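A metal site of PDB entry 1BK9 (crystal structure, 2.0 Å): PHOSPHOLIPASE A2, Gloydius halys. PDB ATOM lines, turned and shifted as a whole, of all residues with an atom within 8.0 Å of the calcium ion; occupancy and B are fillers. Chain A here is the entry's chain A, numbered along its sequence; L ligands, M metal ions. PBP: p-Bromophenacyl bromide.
O of Gly 29 binds the calcium ion, 2.3 Å away. The calcium ion is bound by O of Tyr 27 (2.3 Å). The calcium ion is bound by O of Gly 31. The side-chain carboxylate (OD2) of Asp 48 is bound to the calcium ion (2.5 Å). The calcium ion has four donor atoms within binding distance. Slightly farther from the calcium ion lies the side-chain carboxylate (OD1) of Asp 48 (3.1 Å).
OD1 of Asp 41 lies within hydrogen-bond range of N of Tyr 27 (2.8 Å). SG of Cys 28 is disulfide-bonded to SG of Cys 44 (2.0 Å).
A carbon (CH) of the ligand is bonded to a ring nitrogen (ND1) of His 47, 1.5 Å away.
Trp 30 touches the calcium ion. Five residues have an atom within 4 Å of the calcium ion: Tyr 27, Gly 29, Trp 30, Gly 31 and Asp 48.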
ATOM      1  N   TYR A  21       2.968 -16.160  14.680  1.00  0.00           N
ATOM      2  CA  TYR A  21       2.846 -16.595  16.064  1.00  0.00           C
ATOM      3  C   TYR A  21       4.187 -16.876  16.708  1.00  0.00           C
ATOM      4  O   TYR A  21       4.225 -17.578  17.731  1.00  0.00           O
ATOM      5  CB  TYR A  21       1.975 -17.868  16.091  1.00  0.00           C
ATOM      6  CG  TYR A  21       0.585 -17.657  15.538  1.00  0.00           C
ATOM      7  CD1 TYR A  21      -0.309 -16.916  16.283  1.00  0.00           C
ATOM      8  CD2 TYR A  21       0.251 -18.128  14.297  1.00  0.00           C
ATOM      9  CE1 TYR A  21      -1.564 -16.628  15.786  1.00  0.00           C
ATOM     10  CE2 TYR A  21      -0.989 -17.840  13.800  1.00  0.00           C
ATOM     11  CZ  TYR A  21      -1.883 -17.100  14.546  1.00  0.00           C
ATOM     12  OH  TYR A  21      -3.146 -16.817  14.053  1.00  0.00           O
ATOM     13  N   SER A  22       5.316 -16.383  16.171  1.00  0.00           N
ATOM     14  CA  SER A  22       6.591 -16.749  16.778  1.00  0.00           C
ATOM     15  C   SER A  22       7.123 -15.711  17.766  1.00  0.00           C
ATOM     16  O   SER A  22       8.076 -15.989  18.516  1.00  0.00           O
ATOM     17  CB  SER A  22       7.622 -17.005  15.629  1.00  0.00           C
ATOM     18  OG  SER A  22       7.617 -15.883  14.752  1.00  0.00           O
ATOM     19  N   TYR A  24       4.687 -13.048  19.344  1.00  0.00           N
ATOM     20  CA  TYR A  24       3.498 -12.269  19.606  1.00  0.00           C
ATOM     21  C   TYR A  24       3.172 -12.362  21.116  1.00  0.00           C
ATOM     22  O   TYR A  24       3.056 -13.465  21.689  1.00  0.00           O
ATOM     23  CB  TYR A  24       2.365 -12.832  18.726  1.00  0.00           C
ATOM     24  CG  TYR A  24       0.987 -12.167  18.808  1.00  0.00           C
ATOM     25  CD1 TYR A  24       0.115 -12.382  19.878  1.00  0.00           C
ATOM     26  CD2 TYR A  24       0.578 -11.373  17.761  1.00  0.00           C
ATOM     27  CE1 TYR A  24      -1.130 -11.806  19.915  1.00  0.00           C
ATOM     28  CE2 TYR A  24      -0.674 -10.814  17.786  1.00  0.00           C
ATOM     29  CZ  TYR A  24      -1.503 -11.031  18.858  1.00  0.00           C
ATOM     30  OH  TYR A  24      -2.729 -10.417  18.829  1.00  0.00           O
ATOM     31  N   GLY A  25       3.064 -11.208  21.783  1.00  0.00           N
ATOM     32  CA  GLY A  25       2.693 -11.145  23.188  1.00  0.00           C
ATOM     33  C   GLY A  25       3.745 -11.805  24.065  1.00  0.00           C
ATOM     34  O   GLY A  25       4.923 -11.938  23.716  1.00  0.00           O
ATOM     35  N   CYS A  26       3.347 -12.269  25.242  1.00  0.00           N
ATOM     36  CA  CYS A  26       4.225 -12.906  26.226  1.00  0.00           C
ATOM     37  C   CYS A  26       4.557 -14.358  25.963  1.00  0.00           C
ATOM     38  O   CYS A  26       5.594 -14.876  26.369  1.00  0.00           O
ATOM     39  CB  CYS A  26       3.580 -12.786  27.621  1.00  0.00           C
ATOM     40  SG  CYS A  26       3.403 -11.060  28.167  1.00  0.00           S
ATOM     41  N   TYR A  27       3.652 -15.035  25.261  1.00  0.00           N
ATOM     42  CA  TYR A  27       3.761 -16.467  25.106  1.00  0.00           C
ATOM     43  C   TYR A  27       3.844 -16.986  23.680  1.00  0.00           C
ATOM     44  O   TYR A  27       4.254 -18.141  23.558  1.00  0.00           O
ATOM     45  CB  TYR A  27       2.537 -17.170  25.814  1.00  0.00           C
ATOM     46  CG  TYR A  27       2.686 -17.098  27.331  1.00  0.00           C
ATOM     47  CD1 TYR A  27       3.467 -18.037  27.977  1.00  0.00           C
ATOM     48  CD2 TYR A  27       2.090 -16.060  28.030  1.00  0.00           C
ATOM     49  CE1 TYR A  27       3.693 -17.962  29.342  1.00  0.00           C
ATOM     50  CE2 TYR A  27       2.317 -15.968  29.394  1.00  0.00           C
ATOM     51  CZ  TYR A  27       3.112 -16.907  30.041  1.00  0.00           C
ATOM     52  OH  TYR A  27       3.349 -16.764  31.391  1.00  0.00           O
ATOM     53  N   CYS A  28       3.447 -16.303  22.605  1.00  0.00           N
ATOM     54  CA  CYS A  28       3.553 -16.861  21.272  1.00  0.00           C
ATOM     55  C   CYS A  28       4.985 -16.667  20.803  1.00  0.00           C
ATOM     56  O   CYS A  28       5.406 -15.658  20.255  1.00  0.00           O
ATOM     57  CB  CYS A  28       2.582 -16.172  20.335  1.00  0.00           C
ATOM     58  SG  CYS A  28       0.861 -16.544  20.773  1.00  0.00           S
ATOM     59  N   GLY A  29       5.769 -17.673  21.162  1.00  0.00           N
ATOM     60  CA  GLY A  29       7.180 -17.733  20.897  1.00  0.00           C
ATOM     61  C   GLY A  29       7.768 -18.763  21.837  1.00  0.00           C
ATOM     62  O   GLY A  29       6.999 -19.429  22.547  1.00  0.00           O
ATOM     63  N   TRP A  30       9.067 -18.963  21.904  1.00  0.00           N
ATOM     64  CA  TRP A  30       9.637 -19.972  22.765  1.00  0.00           C
ATOM     65  C   TRP A  30       9.553 -19.477  24.183  1.00  0.00           C
ATOM     66  O   TRP A  30       9.826 -18.307  24.428  1.00  0.00           O
ATOM     67  CB  TRP A  30      11.116 -20.224  22.395  1.00  0.00           C
ATOM     68  CG  TRP A  30      11.580 -21.574  22.924  1.00  0.00           C
ATOM     69  CD1 TRP A  30      12.266 -21.693  24.114  1.00  0.00           C
ATOM     70  CD2 TRP A  30      11.329 -22.780  22.317  1.00  0.00           C
ATOM     71  NE1 TRP A  30      12.438 -22.997  24.253  1.00  0.00           N
ATOM     72  CE2 TRP A  30      11.909 -23.678  23.219  1.00  0.00           C
ATOM     73  CE3 TRP A  30      10.717 -23.219  21.149  1.00  0.00           C
ATOM     74  CZ2 TRP A  30      11.877 -25.032  22.954  1.00  0.00           C
ATOM     75  CZ3 TRP A  30      10.699 -24.562  20.900  1.00  0.00           C
ATOM     76  CH2 TRP A  30      11.266 -25.454  21.785  1.00  0.00           C
ATOM     77  N   GLY A  31       9.155 -20.348  25.116  1.00  0.00           N
ATOM     78  CA  GLY A  31       9.057 -20.026  26.528  1.00  0.00           C
ATOM     79  C   GLY A  31       8.051 -18.921  26.794  1.00  0.00           C
ATOM     80  O   GLY A  31       7.117 -18.726  25.995  1.00  0.00           O
ATOM     81  N   GLY A  32       8.176 -18.173  27.885  1.00  0.00           N
ATOM     82  CA  GLY A  32       7.287 -17.040  28.107  1.00  0.00           C
ATOM     83  C   GLY A  32       7.170 -16.761  29.576  1.00  0.00           C
ATOM     84  O   GLY A  32       7.501 -17.640  30.361  1.00  0.00           O
ATOM     85  N   GLN A  33       6.716 -15.573  29.937  1.00  0.00           N
ATOM     86  CA  GLN A  33       6.501 -15.177  31.328  1.00  0.00           C
ATOM     87  C   GLN A  33       5.379 -14.158  31.257  1.00  0.00           C
ATOM     88  O   GLN A  33       5.022 -13.692  30.171  1.00  0.00           O
ATOM     89  CB  GLN A  33       7.617 -14.377  32.015  1.00  0.00           C
ATOM     90  CG  GLN A  33       9.105 -14.630  31.936  1.00  0.00           C
ATOM     91  CD  GLN A  33       9.881 -13.713  30.973  1.00  0.00           C
ATOM     92  OE1 GLN A  33      10.899 -14.164  30.423  1.00  0.00           O
ATOM     93  NE2 GLN A  33       9.529 -12.451  30.714  1.00  0.00           N
ATOM     94  N   ASP A  41      -2.605 -14.958  22.491  1.00  0.00           N
ATOM     95  CA  ASP A  41      -1.538 -15.205  23.445  1.00  0.00           C
ATOM     96  C   ASP A  41      -1.921 -16.288  24.476  1.00  0.00           C
ATOM     97  O   ASP A  41      -1.088 -17.098  24.887  1.00  0.00           O
ATOM     98  CB  ASP A  41      -1.182 -13.902  24.180  1.00  0.00           C
ATOM     99  CG  ASP A  41       0.270 -13.880  24.683  1.00  0.00           C
ATOM    100  OD1 ASP A  41       1.114 -14.660  24.243  1.00  0.00           O
ATOM    101  OD2 ASP A  41       0.564 -13.073  25.543  1.00  0.00           O
ATOM    102  N   CYS A  44      -1.355 -19.645  23.001  1.00  0.00           N
ATOM    103  CA  CYS A  44       0.040 -20.074  23.092  1.00  0.00           C
ATOM    104  C   CYS A  44       0.434 -20.515  24.486  1.00  0.00           C
ATOM    105  O   CYS A  44       1.208 -21.457  24.658  1.00  0.00           O
ATOM    106  CB  CYS A  44       0.991 -18.973  22.682  1.00  0.00           C
ATOM    107  SG  CYS A  44       0.817 -18.560  20.935  1.00  0.00           S
ATOM    108  N   PHE A  45      -0.084 -19.822  25.499  1.00  0.00           N
ATOM    109  CA  PHE A  45       0.158 -20.164  26.891  1.00  0.00           C
ATOM    110  C   PHE A  45      -0.347 -21.578  27.167  1.00  0.00           C
ATOM    111  O   PHE A  45       0.371 -22.370  27.790  1.00  0.00           O
ATOM    112  CB  PHE A  45      -0.584 -19.158  27.826  1.00  0.00           C
ATOM    113  CG  PHE A  45      -0.667 -19.521  29.331  1.00  0.00           C
ATOM    114  CD1 PHE A  45       0.461 -19.493  30.139  1.00  0.00           C
ATOM    115  CD2 PHE A  45      -1.896 -19.847  29.903  1.00  0.00           C
ATOM    116  CE1 PHE A  45       0.359 -19.791  31.494  1.00  0.00           C
ATOM    117  CE2 PHE A  45      -1.983 -20.140  31.267  1.00  0.00           C
ATOM    118  CZ  PHE A  45      -0.856 -20.117  32.067  1.00  0.00           C
ATOM    119  N   VAL A  46      -1.567 -21.915  26.706  1.00  0.00           N
ATOM    120  CA  VAL A  46      -2.131 -23.234  26.972  1.00  0.00           C
ATOM    121  C   VAL A  46      -1.277 -24.250  26.235  1.00  0.00           C
ATOM    122  O   VAL A  46      -0.973 -25.297  26.819  1.00  0.00           O
ATOM    123  CB  VAL A  46      -3.645 -23.314  26.526  1.00  0.00           C
ATOM    124  CG1 VAL A  46      -4.199 -24.756  26.597  1.00  0.00           C
ATOM    125  CG2 VAL A  46      -4.486 -22.442  27.498  1.00  0.00           C
ATOM    126  N   HIS A  47      -0.813 -23.935  25.009  1.00  0.00           N
ATOM    127  CA  HIS A  47       0.019 -24.835  24.233  1.00  0.00           C
ATOM    128  C   HIS A  47       1.334 -25.130  24.962  1.00  0.00           C
ATOM    129  O   HIS A  47       1.803 -26.279  24.936  1.00  0.00           O
ATOM    130  CB  HIS A  47       0.285 -24.205  22.829  1.00  0.00           C
ATOM    131  CG  HIS A  47       1.097 -25.087  21.888  1.00  0.00           C
ATOM    132  ND1 HIS A  47       2.408 -24.955  21.690  1.00  0.00           N
ATOM    133  CD2 HIS A  47       0.585 -26.162  21.217  1.00  0.00           C
ATOM    134  CE1 HIS A  47       2.705 -25.948  20.891  1.00  0.00           C
ATOM    135  NE2 HIS A  47       1.639 -26.644  20.616  1.00  0.00           N
ATOM    136  N   ASP A  48       1.960 -24.102  25.583  1.00  0.00           N
ATOM    137  CA  ASP A  48       3.155 -24.266  26.437  1.00  0.00           C
ATOM    138  C   ASP A  48       2.922 -25.166  27.620  1.00  0.00           C
ATOM    139  O   ASP A  48       3.736 -26.036  27.914  1.00  0.00           O
ATOM    140  CB  ASP A  48       3.633 -22.945  26.997  1.00  0.00           C
ATOM    141  CG  ASP A  48       4.402 -22.093  25.982  1.00  0.00           C
ATOM    142  OD1 ASP A  48       4.856 -22.626  24.961  1.00  0.00           O
ATOM    143  OD2 ASP A  48       4.527 -20.887  26.249  1.00  0.00           O
ATOM    144  N   CYS A  49       1.781 -24.971  28.300  1.00  0.00           N
ATOM    145  CA  CYS A  49       1.434 -25.786  29.430  1.00  0.00           C
ATOM    146  C   CYS A  49       1.195 -27.225  28.962  1.00  0.00           C
ATOM    147  O   CYS A  49       1.664 -28.162  29.603  1.00  0.00           O
ATOM    148  CB  CYS A  49       0.159 -25.281  30.073  1.00  0.00           C
ATOM    149  SG  CYS A  49       0.285 -23.610  30.765  1.00  0.00           S
HETATM  150  CH  PBP L   1       3.234 -23.854  22.183  1.00  0.00           C
HETATM  151  CG  PBP L   1       4.375 -22.026  20.733  1.00  0.00           C
HETATM  152  CD1 PBP L   1       4.283 -21.018  19.791  1.00  0.00           C
HETATM  153  CE1 PBP L   1       5.408 -20.556  19.153  1.00  0.00           C
HETATM  154  CD2 PBP L   1       5.622 -22.552  21.022  1.00  0.00           C
HETATM  155  CE2 PBP L   1       6.762 -22.097  20.376  1.00  0.00           C
HETATM  156  CZ  PBP L   1       6.669 -21.089  19.434  1.00  0.00           C
HETATM  157 BR   PBP L   1       8.203 -20.523  18.470  1.00  0.00          BR
HETATM  158  CR  PBP L   1       3.228 -22.641  21.249  1.00  0.00           C
HETATM  159  O   PBP L   1       2.129 -22.199  20.900  1.00  0.00           O
HETATM  160 CA    CA M   1       5.712 -19.739  24.424  1.00  0.00          CA
